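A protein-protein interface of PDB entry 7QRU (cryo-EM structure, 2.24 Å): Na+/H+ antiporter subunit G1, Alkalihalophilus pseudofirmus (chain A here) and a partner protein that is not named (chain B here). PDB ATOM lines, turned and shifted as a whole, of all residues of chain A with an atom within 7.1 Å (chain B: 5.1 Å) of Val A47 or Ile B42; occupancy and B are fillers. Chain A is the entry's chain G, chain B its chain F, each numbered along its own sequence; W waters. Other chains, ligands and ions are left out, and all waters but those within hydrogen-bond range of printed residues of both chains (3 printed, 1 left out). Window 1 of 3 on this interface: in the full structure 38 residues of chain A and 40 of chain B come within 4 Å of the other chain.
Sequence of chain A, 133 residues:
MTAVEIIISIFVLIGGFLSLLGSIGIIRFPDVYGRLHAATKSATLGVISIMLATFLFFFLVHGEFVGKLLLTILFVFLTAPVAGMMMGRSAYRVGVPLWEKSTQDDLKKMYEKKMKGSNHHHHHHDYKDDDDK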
ATOM      1  N   ILE A  14       1.794  12.534 -18.749  1.00  0.00           N
ATOM      2  CA  ILE A  14       0.386  12.229 -18.938  1.00  0.00           C
ATOM      3  C   ILE A  14       0.010  12.368 -20.418  1.00  0.00           C
ATOM      4  O   ILE A  14      -0.757  11.584 -20.956  1.00  0.00           O
ATOM      5  CB  ILE A  14      -0.462  13.150 -18.046  1.00  0.00           C
ATOM      6  CG1 ILE A  14      -0.233  12.791 -16.581  1.00  0.00           C
ATOM      7  CG2 ILE A  14      -1.926  13.127 -18.413  1.00  0.00           C
ATOM      8  CD1 ILE A  14      -0.756  13.877 -15.656  1.00  0.00           C
ATOM      9  N   GLY A  15       0.434  13.433 -21.059  1.00  0.00           N
ATOM     10  CA  GLY A  15       0.004  13.656 -22.404  1.00  0.00           C
ATOM     11  C   GLY A  15       0.488  12.555 -23.343  1.00  0.00           C
ATOM     12  O   GLY A  15      -0.255  12.142 -24.196  1.00  0.00           O
ATOM     13  N   GLY A  16       1.684  12.086 -23.134  1.00  0.00           N
ATOM     14  CA  GLY A  16       2.214  11.046 -23.973  1.00  0.00           C
ATOM     15  C   GLY A  16       1.590   9.686 -23.721  1.00  0.00           C
ATOM     16  O   GLY A  16       1.163   9.047 -24.653  1.00  0.00           O
ATOM     17  N   LEU A  18      -1.561   9.365 -22.497  1.00  0.00           N
ATOM     18  CA  LEU A  18      -2.928   9.325 -22.964  1.00  0.00           C
ATOM     19  C   LEU A  18      -2.962   9.233 -24.485  1.00  0.00           C
ATOM     20  O   LEU A  18      -3.943   8.746 -25.025  1.00  0.00           O
ATOM     21  CB  LEU A  18      -3.780  10.516 -22.500  1.00  0.00           C
ATOM     22  CG  LEU A  18      -3.977  10.575 -21.010  1.00  0.00           C
ATOM     23  CD1 LEU A  18      -4.511  11.927 -20.619  1.00  0.00           C
ATOM     24  CD2 LEU A  18      -4.811   9.419 -20.554  1.00  0.00           C
ATOM     25  N   SER A  19      -2.002   9.783 -25.186  1.00  0.00           N
ATOM     26  CA  SER A  19      -1.937   9.626 -26.629  1.00  0.00           C
ATOM     27  C   SER A  19      -1.818   8.155 -27.013  1.00  0.00           C
ATOM     28  O   SER A  19      -2.450   7.718 -27.935  1.00  0.00           O
ATOM     29  CB  SER A  19      -0.740  10.407 -27.173  1.00  0.00           C
ATOM     30  OG  SER A  19      -0.943  11.813 -26.865  1.00  0.00           O
ATOM     31  N   ALA A  39     -10.617   7.947 -29.536  1.00  0.00           N
ATOM     32  CA  ALA A  39     -10.146   8.996 -30.392  1.00  0.00           C
ATOM     33  C   ALA A  39     -10.581  10.366 -29.866  1.00  0.00           C
ATOM     34  O   ALA A  39      -9.762  11.201 -29.543  1.00  0.00           O
ATOM     35  CB  ALA A  39     -10.649   8.774 -31.784  1.00  0.00           C
ATOM     36  N   LYS A  41     -11.687  11.146 -26.766  1.00  0.00           N
ATOM     37  CA  LYS A  41     -11.392  11.522 -25.382  1.00  0.00           C
ATOM     38  C   LYS A  41      -9.886  11.496 -25.093  1.00  0.00           C
ATOM     39  O   LYS A  41      -9.371  12.440 -24.549  1.00  0.00           O
ATOM     40  CB  LYS A  41     -12.089  10.617 -24.388  1.00  0.00           C
ATOM     41  CG  LYS A  41     -13.573  10.880 -24.511  1.00  0.00           C
ATOM     42  CD  LYS A  41     -14.472   9.764 -24.016  1.00  0.00           C
ATOM     43  CE  LYS A  41     -15.893  10.197 -24.300  1.00  0.00           C
ATOM     44  NZ  LYS A  41     -16.677   9.082 -23.832  1.00  0.00           N
ATOM     45  N   SER A  42      -9.178  10.386 -25.391  1.00  0.00           N
ATOM     46  CA  SER A  42      -7.783  10.237 -24.995  1.00  0.00           C
ATOM     47  C   SER A  42      -6.875  11.067 -25.881  1.00  0.00           C
ATOM     48  O   SER A  42      -6.019  11.779 -25.395  1.00  0.00           O
ATOM     49  CB  SER A  42      -7.388   8.792 -24.936  1.00  0.00           C
ATOM     50  OG  SER A  42      -8.174   8.187 -23.953  1.00  0.00           O
ATOM     51  N   ALA A  43      -7.050  10.938 -27.173  1.00  0.00           N
ATOM     52  CA  ALA A  43      -6.237  11.730 -28.064  1.00  0.00           C
ATOM     53  C   ALA A  43      -6.436  13.219 -27.687  1.00  0.00           C
ATOM     54  O   ALA A  43      -5.520  14.026 -27.679  1.00  0.00           O
ATOM     55  CB  ALA A  43      -6.597  11.428 -29.536  1.00  0.00           C
ATOM     56  N   THR A  44      -7.674  13.614 -27.442  1.00  0.00           N
ATOM     57  CA  THR A  44      -7.937  14.971 -27.046  1.00  0.00           C
ATOM     58  C   THR A  44      -7.273  15.382 -25.726  1.00  0.00           C
ATOM     59  O   THR A  44      -6.657  16.425 -25.747  1.00  0.00           O
ATOM     60  CB  THR A  44      -9.437  15.167 -26.934  1.00  0.00           C
ATOM     61  OG1 THR A  44      -9.846  14.878 -28.261  1.00  0.00           O
ATOM     62  CG2 THR A  44      -9.834  16.580 -26.596  1.00  0.00           C
ATOM     63  N   LEU A  45      -7.486  14.723 -24.574  1.00  0.00           N
ATOM     64  CA  LEU A  45      -6.788  15.089 -23.355  1.00  0.00           C
ATOM     65  C   LEU A  45      -5.257  14.955 -23.438  1.00  0.00           C
ATOM     66  O   LEU A  45      -4.512  15.808 -22.953  1.00  0.00           O
ATOM     67  CB  LEU A  45      -7.286  14.219 -22.213  1.00  0.00           C
ATOM     68  CG  LEU A  45      -6.842  14.679 -20.817  1.00  0.00           C
ATOM     69  CD1 LEU A  45      -7.259  16.077 -20.556  1.00  0.00           C
ATOM     70  CD2 LEU A  45      -7.459  13.811 -19.734  1.00  0.00           C
ATOM     71  N   GLY A  46      -4.771  13.967 -24.139  1.00  0.00           N
ATOM     72  CA  GLY A  46      -3.352  13.807 -24.334  1.00  0.00           C
ATOM     73  C   GLY A  46      -2.756  15.031 -24.951  1.00  0.00           C
ATOM     74  O   GLY A  46      -1.691  15.477 -24.546  1.00  0.00           O
ATOM     75  N   VAL A  47      -3.414  15.558 -25.960  1.00  0.00           N
ATOM     76  CA  VAL A  47      -2.838  16.678 -26.710  1.00  0.00           C
ATOM     77  C   VAL A  47      -3.083  17.939 -25.905  1.00  0.00           C
ATOM     78  O   VAL A  47      -2.192  18.764 -25.802  1.00  0.00           O
ATOM     79  CB  VAL A  47      -3.400  16.791 -28.162  1.00  0.00           C
ATOM     80  CG1 VAL A  47      -4.806  17.334 -28.229  1.00  0.00           C
ATOM     81  CG2 VAL A  47      -2.647  17.704 -29.020  1.00  0.00           C
ATOM     82  N   ILE A  48      -4.227  18.046 -25.198  1.00  0.00           N
ATOM     83  CA  ILE A  48      -4.385  19.183 -24.300  1.00  0.00           C
ATOM     84  C   ILE A  48      -3.303  19.244 -23.237  1.00  0.00           C
ATOM     85  O   ILE A  48      -2.779  20.299 -22.974  1.00  0.00           O
ATOM     86  CB  ILE A  48      -5.767  19.239 -23.714  1.00  0.00           C
ATOM     87  CG1 ILE A  48      -6.714  19.589 -24.872  1.00  0.00           C
ATOM     88  CG2 ILE A  48      -5.808  20.249 -22.588  1.00  0.00           C
ATOM     89  CD1 ILE A  48      -8.198  19.272 -24.606  1.00  0.00           C
ATOM     90  N   SER A  49      -2.893  18.118 -22.698  1.00  0.00           N
ATOM     91  CA  SER A  49      -1.922  18.070 -21.624  1.00  0.00           C
ATOM     92  C   SER A  49      -0.544  18.444 -22.122  1.00  0.00           C
ATOM     93  O   SER A  49       0.146  19.197 -21.466  1.00  0.00           O
ATOM     94  CB  SER A  49      -1.946  16.653 -20.922  1.00  0.00           C
ATOM     95  OG  SER A  49      -0.761  16.455 -20.141  1.00  0.00           O
ATOM     96  N   ILE A  50      -0.141  17.972 -23.284  1.00  0.00           N
ATOM     97  CA  ILE A  50       1.099  18.451 -23.887  1.00  0.00           C
ATOM     98  C   ILE A  50       1.106  19.947 -24.239  1.00  0.00           C
ATOM     99  O   ILE A  50       2.093  20.597 -23.958  1.00  0.00           O
ATOM    100  CB  ILE A  50       1.462  17.558 -25.099  1.00  0.00           C
ATOM    101  CG1 ILE A  50       1.831  16.148 -24.621  1.00  0.00           C
ATOM    102  CG2 ILE A  50       2.581  18.154 -25.916  1.00  0.00           C
ATOM    103  CD1 ILE A  50       1.842  15.195 -25.718  1.00  0.00           C
ATOM    104  N   MET A  51       0.022  20.513 -24.731  1.00  0.00           N
ATOM    105  CA  MET A  51       0.011  21.926 -25.001  1.00  0.00           C
ATOM    106  C   MET A  51       0.113  22.697 -23.692  1.00  0.00           C
ATOM    107  O   MET A  51       0.749  23.703 -23.657  1.00  0.00           O
ATOM    108  CB  MET A  51      -1.255  22.377 -25.686  1.00  0.00           C
ATOM    109  CG  MET A  51      -1.472  21.800 -27.183  1.00  0.00           C
ATOM    110  SD  MET A  51      -0.353  22.660 -28.268  1.00  0.00           S
ATOM    111  CE  MET A  51       1.133  21.671 -28.242  1.00  0.00           C
ATOM    112  N   LEU A  52      -0.561  22.302 -22.631  1.00  0.00           N
ATOM    113  CA  LEU A  52      -0.291  22.912 -21.357  1.00  0.00           C
ATOM    114  C   LEU A  52       1.185  22.840 -20.970  1.00  0.00           C
ATOM    115  O   LEU A  52       1.636  23.811 -20.424  1.00  0.00           O
ATOM    116  CB  LEU A  52      -1.130  22.230 -20.287  1.00  0.00           C
ATOM    117  CG  LEU A  52      -2.520  22.763 -20.222  1.00  0.00           C
ATOM    118  CD1 LEU A  52      -3.265  21.928 -19.227  1.00  0.00           C
ATOM    119  CD2 LEU A  52      -2.436  24.222 -19.821  1.00  0.00           C
ATOM    120  N   ALA A  53       1.847  21.702 -21.044  1.00  0.00           N
ATOM    121  CA  ALA A  53       3.243  21.561 -20.667  1.00  0.00           C
ATOM    122  C   ALA A  53       4.043  22.547 -21.496  1.00  0.00           C
ATOM    123  O   ALA A  53       4.828  23.306 -20.988  1.00  0.00           O
ATOM    124  CB  ALA A  53       3.736  20.101 -20.909  1.00  0.00           C
ATOM    125  N   THR A  54       3.775  22.593 -22.797  1.00  0.00           N
ATOM    126  CA  THR A  54       4.512  23.481 -23.675  1.00  0.00           C
ATOM    127  C   THR A  54       4.227  24.907 -23.262  1.00  0.00           C
ATOM    128  O   THR A  54       5.125  25.705 -23.156  1.00  0.00           O
ATOM    129  CB  THR A  54       4.132  23.216 -25.127  1.00  0.00           C
ATOM    130  OG1 THR A  54       4.124  21.791 -25.304  1.00  0.00           O
ATOM    131  CG2 THR A  54       5.106  23.865 -26.055  1.00  0.00           C
ATOM    132  N   THR A  72      -4.698  26.780 -29.555  1.00  0.00           N
ATOM    133  CA  THR A  72      -4.753  25.393 -29.986  1.00  0.00           C
ATOM    134  C   THR A  72      -5.599  24.562 -29.007  1.00  0.00           C
ATOM    135  O   THR A  72      -6.299  23.712 -29.456  1.00  0.00           O
ATOM    136  CB  THR A  72      -3.366  24.798 -30.126  1.00  0.00           C
ATOM    137  OG1 THR A  72      -2.650  25.671 -30.985  1.00  0.00           O
ATOM    138  CG2 THR A  72      -3.420  23.404 -30.689  1.00  0.00           C
ATOM    139  N   ILE A  73      -5.474  24.710 -27.688  1.00  0.00           N
ATOM    140  CA  ILE A  73      -6.344  23.971 -26.790  1.00  0.00           C
ATOM    141  C   ILE A  73      -7.810  24.192 -27.100  1.00  0.00           C
ATOM    142  O   ILE A  73      -8.591  23.254 -27.050  1.00  0.00           O
ATOM    143  CB  ILE A  73      -6.044  24.275 -25.321  1.00  0.00           C
ATOM    144  CG1 ILE A  73      -4.653  23.696 -25.044  1.00  0.00           C
ATOM    145  CG2 ILE A  73      -7.076  23.662 -24.418  1.00  0.00           C
ATOM    146  CD1 ILE A  73      -4.068  24.230 -23.850  1.00  0.00           C
ATOM    147  N   VAL A  76      -8.893  22.388 -30.379  1.00  0.00           N
ATOM    148  CA  VAL A  76      -9.058  20.966 -30.082  1.00  0.00           C
ATOM    149  C   VAL A  76     -10.347  20.690 -29.295  1.00  0.00           C
ATOM    150  O   VAL A  76     -11.098  19.819 -29.690  1.00  0.00           O
ATOM    151  CB  VAL A  76      -7.820  20.387 -29.388  1.00  0.00           C
ATOM    152  CG1 VAL A  76      -8.151  18.992 -28.918  1.00  0.00           C
ATOM    153  CG2 VAL A  76      -6.605  20.412 -30.315  1.00  0.00           C
ATOM    154  N   THR A  79     -13.590  21.250 -31.676  1.00  0.00           N
ATOM    155  CA  THR A  79     -13.557  20.461 -32.874  1.00  0.00           C
ATOM    156  C   THR A  79     -13.715  18.983 -32.543  1.00  0.00           C
ATOM    157  O   THR A  79     -14.321  18.280 -33.328  1.00  0.00           O
ATOM    158  CB  THR A  79     -12.200  20.751 -33.549  1.00  0.00           C
ATOM    159  OG1 THR A  79     -12.492  21.795 -34.518  1.00  0.00           O
ATOM    160  CG2 THR A  79     -11.543  19.483 -34.061  1.00  0.00           C
ATOM    161  N   ALA A  80     -13.142  18.483 -31.436  1.00  0.00           N
ATOM    162  CA  ALA A  80     -13.105  17.053 -31.139  1.00  0.00           C
ATOM    163  C   ALA A  80     -14.531  16.475 -31.074  1.00  0.00           C
ATOM    164  O   ALA A  80     -14.852  15.525 -31.719  1.00  0.00           O
ATOM    165  CB  ALA A  80     -12.433  16.804 -29.839  1.00  0.00           C
ATOM    166  N   ASP B  38      -7.827  10.811 -38.309  1.00  0.00           N
ATOM    167  CA  ASP B  38      -8.146  11.942 -37.479  1.00  0.00           C
ATOM    168  C   ASP B  38      -7.277  11.847 -36.226  1.00  0.00           C
ATOM    169  O   ASP B  38      -6.745  12.826 -35.728  1.00  0.00           O
ATOM    170  CB  ASP B  38      -9.646  11.971 -37.139  1.00  0.00           C
ATOM    171  CG  ASP B  38      -9.936  12.880 -35.950  1.00  0.00           C
ATOM    172  OD1 ASP B  38      -9.928  14.191 -36.123  1.00  0.00           O
ATOM    173  OD2 ASP B  38     -10.070  12.284 -34.824  1.00  0.00           O
ATOM    174  N   THR B  39      -7.189  10.673 -35.636  1.00  0.00           N
ATOM    175  CA  THR B  39      -6.348  10.512 -34.449  1.00  0.00           C
ATOM    176  C   THR B  39      -4.838  10.693 -34.746  1.00  0.00           C
ATOM    177  O   THR B  39      -4.107  11.289 -33.963  1.00  0.00           O
ATOM    178  CB  THR B  39      -6.590   9.143 -33.844  1.00  0.00           C
ATOM    179  OG1 THR B  39      -8.012   8.932 -33.890  1.00  0.00           O
ATOM    180  CG2 THR B  39      -6.019   8.999 -32.470  1.00  0.00           C
ATOM    181  N   PHE B  40      -4.375  10.313 -35.942  1.00  0.00           N
ATOM    182  CA  PHE B  40      -2.991  10.473 -36.349  1.00  0.00           C
ATOM    183  C   PHE B  40      -2.650  11.964 -36.315  1.00  0.00           C
ATOM    184  O   PHE B  40      -1.569  12.368 -35.874  1.00  0.00           O
ATOM    185  CB  PHE B  40      -2.823   9.851 -37.753  1.00  0.00           C
ATOM    186  CG  PHE B  40      -1.388   9.707 -38.222  1.00  0.00           C
ATOM    187  CD1 PHE B  40      -0.742  10.744 -38.864  1.00  0.00           C
ATOM    188  CD2 PHE B  40      -0.710   8.515 -38.080  1.00  0.00           C
ATOM    189  CE1 PHE B  40       0.554  10.614 -39.315  1.00  0.00           C
ATOM    190  CE2 PHE B  40       0.604   8.387 -38.489  1.00  0.00           C
ATOM    191  CZ  PHE B  40       1.243   9.439 -39.089  1.00  0.00           C
ATOM    192  N   GLY B  41      -3.531  12.809 -36.889  1.00  0.00           N
ATOM    193  CA  GLY B  41      -3.254  14.216 -36.986  1.00  0.00           C
ATOM    194  C   GLY B  41      -3.269  14.911 -35.638  1.00  0.00           C
ATOM    195  O   GLY B  41      -2.406  15.746 -35.353  1.00  0.00           O
ATOM    196  N   ILE B  42      -4.239  14.563 -34.790  1.00  0.00           N
ATOM    197  CA  ILE B  42      -4.249  15.104 -33.422  1.00  0.00           C
ATOM    198  C   ILE B  42      -2.944  14.762 -32.705  1.00  0.00           C
ATOM    199  O   ILE B  42      -2.396  15.637 -32.037  1.00  0.00           O
ATOM    200  CB  ILE B  42      -5.499  14.610 -32.663  1.00  0.00           C
ATOM    201  CG1 ILE B  42      -6.754  15.174 -33.370  1.00  0.00           C
ATOM    202  CG2 ILE B  42      -5.489  14.924 -31.189  1.00  0.00           C
ATOM    203  CD1 ILE B  42      -6.691  16.699 -33.538  1.00  0.00           C
ATOM    204  N   ASN B  43      -2.474  13.523 -32.831  1.00  0.00           N
ATOM    205  CA  ASN B  43      -1.246  13.101 -32.175  1.00  0.00           C
ATOM    206  C   ASN B  43      -0.023  13.879 -32.657  1.00  0.00           C
ATOM    207  O   ASN B  43       0.886  14.112 -31.863  1.00  0.00           O
ATOM    208  CB  ASN B  43      -0.998  11.568 -32.277  1.00  0.00           C
ATOM    209  CG  ASN B  43      -1.963  10.773 -31.377  1.00  0.00           C
ATOM    210  OD1 ASN B  43      -2.248   9.597 -31.575  1.00  0.00           O
ATOM    211  ND2 ASN B  43      -2.651  11.440 -30.477  1.00  0.00           N
ATOM    212  N   LEU B  44      -0.003  14.294 -33.930  1.00  0.00           N
ATOM    213  CA  LEU B  44       1.053  15.155 -34.424  1.00  0.00           C
ATOM    214  C   LEU B  44       1.191  16.474 -33.670  1.00  0.00           C
ATOM    215  O   LEU B  44       2.288  16.916 -33.401  1.00  0.00           O
ATOM    216  CB  LEU B  44       0.810  15.448 -35.894  1.00  0.00           C
ATOM    217  CG  LEU B  44       1.123  14.351 -36.901  1.00  0.00           C
ATOM    218  CD1 LEU B  44       1.016  15.020 -38.241  1.00  0.00           C
ATOM    219  CD2 LEU B  44       2.481  13.755 -36.669  1.00  0.00           C
ATOM    220  N   ILE B  45       0.092  17.068 -33.224  1.00  0.00           N
ATOM    221  CA  ILE B  45       0.177  18.258 -32.371  1.00  0.00           C
ATOM    222  C   ILE B  45       0.958  17.984 -31.090  1.00  0.00           C
ATOM    223  O   ILE B  45       1.810  18.784 -30.730  1.00  0.00           O
ATOM    224  CB  ILE B  45      -1.220  18.781 -31.986  1.00  0.00           C
ATOM    225  CG1 ILE B  45      -2.054  19.054 -33.221  1.00  0.00           C
ATOM    226  CG2 ILE B  45      -1.123  19.958 -31.048  1.00  0.00           C
ATOM    227  CD1 ILE B  45      -3.436  19.298 -32.825  1.00  0.00           C
ATOM    228  N   GLY B  46       0.716  16.803 -30.457  1.00  0.00           N
ATOM    229  CA  GLY B  46       1.468  16.413 -29.282  1.00  0.00           C
ATOM    230  C   GLY B  46       2.960  16.372 -29.610  1.00  0.00           C
ATOM    231  O   GLY B  46       3.829  16.890 -28.896  1.00  0.00           O
ATOM    232  N   ILE B  67      -2.367  22.333 -37.778  1.00  0.00           N
ATOM    233  CA  ILE B  67      -2.695  20.925 -37.825  1.00  0.00           C
ATOM    234  C   ILE B  67      -4.080  20.744 -37.232  1.00  0.00           C
ATOM    235  O   ILE B  67      -4.859  19.958 -37.713  1.00  0.00           O
ATOM    236  CB  ILE B  67      -1.672  20.061 -37.068  1.00  0.00           C
ATOM    237  CG1 ILE B  67      -0.360  19.985 -37.785  1.00  0.00           C
ATOM    238  CG2 ILE B  67      -2.239  18.683 -36.768  1.00  0.00           C
ATOM    239  CD1 ILE B  67       0.706  19.525 -36.860  1.00  0.00           C
ATOM    240  N   SER B  68      -4.355  21.379 -36.109  1.00  0.00           N
ATOM    241  CA  SER B  68      -5.668  21.204 -35.521  1.00  0.00           C
ATOM    242  C   SER B  68      -6.773  21.607 -36.520  1.00  0.00           C
ATOM    243  O   SER B  68      -7.727  20.891 -36.698  1.00  0.00           O
ATOM    244  CB  SER B  68      -5.680  21.972 -34.231  1.00  0.00           C
ATOM    245  OG  SER B  68      -5.892  23.344 -34.450  1.00  0.00           O
ATOM    246  N   ALA B  71      -6.720  18.860 -39.574  1.00  0.00           N
ATOM    247  CA  ALA B  71      -7.208  17.541 -39.245  1.00  0.00           C
ATOM    248  C   ALA B  71      -8.747  17.552 -39.218  1.00  0.00           C
ATOM    249  O   ALA B  71      -9.408  16.619 -39.699  1.00  0.00           O
ATOM    250  CB  ALA B  71      -6.683  17.041 -37.950  1.00  0.00           C
HETATM  251  O   HOH W   1      -8.736  12.236 -32.424  1.00  0.00           O
HETATM  252  O   HOH W   2      -3.948   8.659 -29.855  1.00  0.00           O
HETATM  253  O   HOH W   3      -3.290  12.697 -27.882  1.00  0.00           O
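OD1 of Asn B43 lies close to O of Thr B39 (3.5 Å).
The backbone carbonyl oxygen (O) of Ile A50 is in hydrogen-bond range of the side-chain hydroxyl (OG1) of Thr A54.
The side-chain hydroxyl (OG) of Ser A19 sits at hydrogen-bond distance from the backbone carbonyl oxygen (O) of Gly A15, 2.8 Å away.
CB of Ser A19 touches ND2 of Asn B43, 3.95 Å away.
Ala A39 touches Thr B39.
Ala A43 touches Thr B39 (CB to CG2, 3.9 Å).
Ala A43 touches Ile B42 (O to CG2, 3.6 Å).
Ile B42 touches Val A47.
Ile B45 touches Val A47 (CG2 to CG2, 3.4 Å).
CG2 of Val A47 touches N of Gly B46, at 3.8 Å.
O of Gly B46 touches CG2 of Ile A50, at 3.5 Å.
Met A51 touches Ile B45.
Printed residues of chain B within 4 Å of Ser A19: Asn B43 (3.95 Å).
Of the printed residues of chain B, Ala A43 touches Thr B39 and Ile B42.
Of chain B, only Ile B42, Ile B45 and Gly B46 come within 4 Å of Val A47.
No residue of chain A comes within 4 Å of Gly B41.
Printed residues of chain A within 4 Å of Asn B43: Ser A19 (3.95 Å).
Printed residues of chain A within 4 Å of Ile B45: Val A47 (3.4 Å) and Met A51 (3.9 Å).
Ile B67 touches none of the printed residues of chain A.
The nearest residue of chain A that does not touch Ile B42 is Thr A44 (4.5 Å).
Hydrophobic or aromatic side chains of chain B within 4 Å of the printed part of chain A: Ile B42 and Ile B45.
Printed residues of chain A that touch a printed residue of chain B: Ser A19, Ala A39, Ala A43, Val A47, Ile A50 and Met A51.
Hydrophobic or aromatic side chains of chain A within 4 Å of the printed part of chain B: Ala A39, Ala A43, Val A47, Ile A50 and Met A51.
Among the printed residues, no Asp or Glu carboxylate lies within 4 Å of a Lys or Arg side-chain nitrogen of the other chain.
Water W2 bridges the side-chain amide oxygen of Asn B43 and the backbone carbonyl oxygen of Ser A19.
Water W3 lies within hydrogen-bond range of O of Ala A43, OG of Ser A19, ND2 of Asn B43 and N of Val A47.
Water W1 bridges the side-chain carboxylate of Asp B38 (2.7 Å) and the backbone carbonyl oxygen of Ala A39 (3.2 Å).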
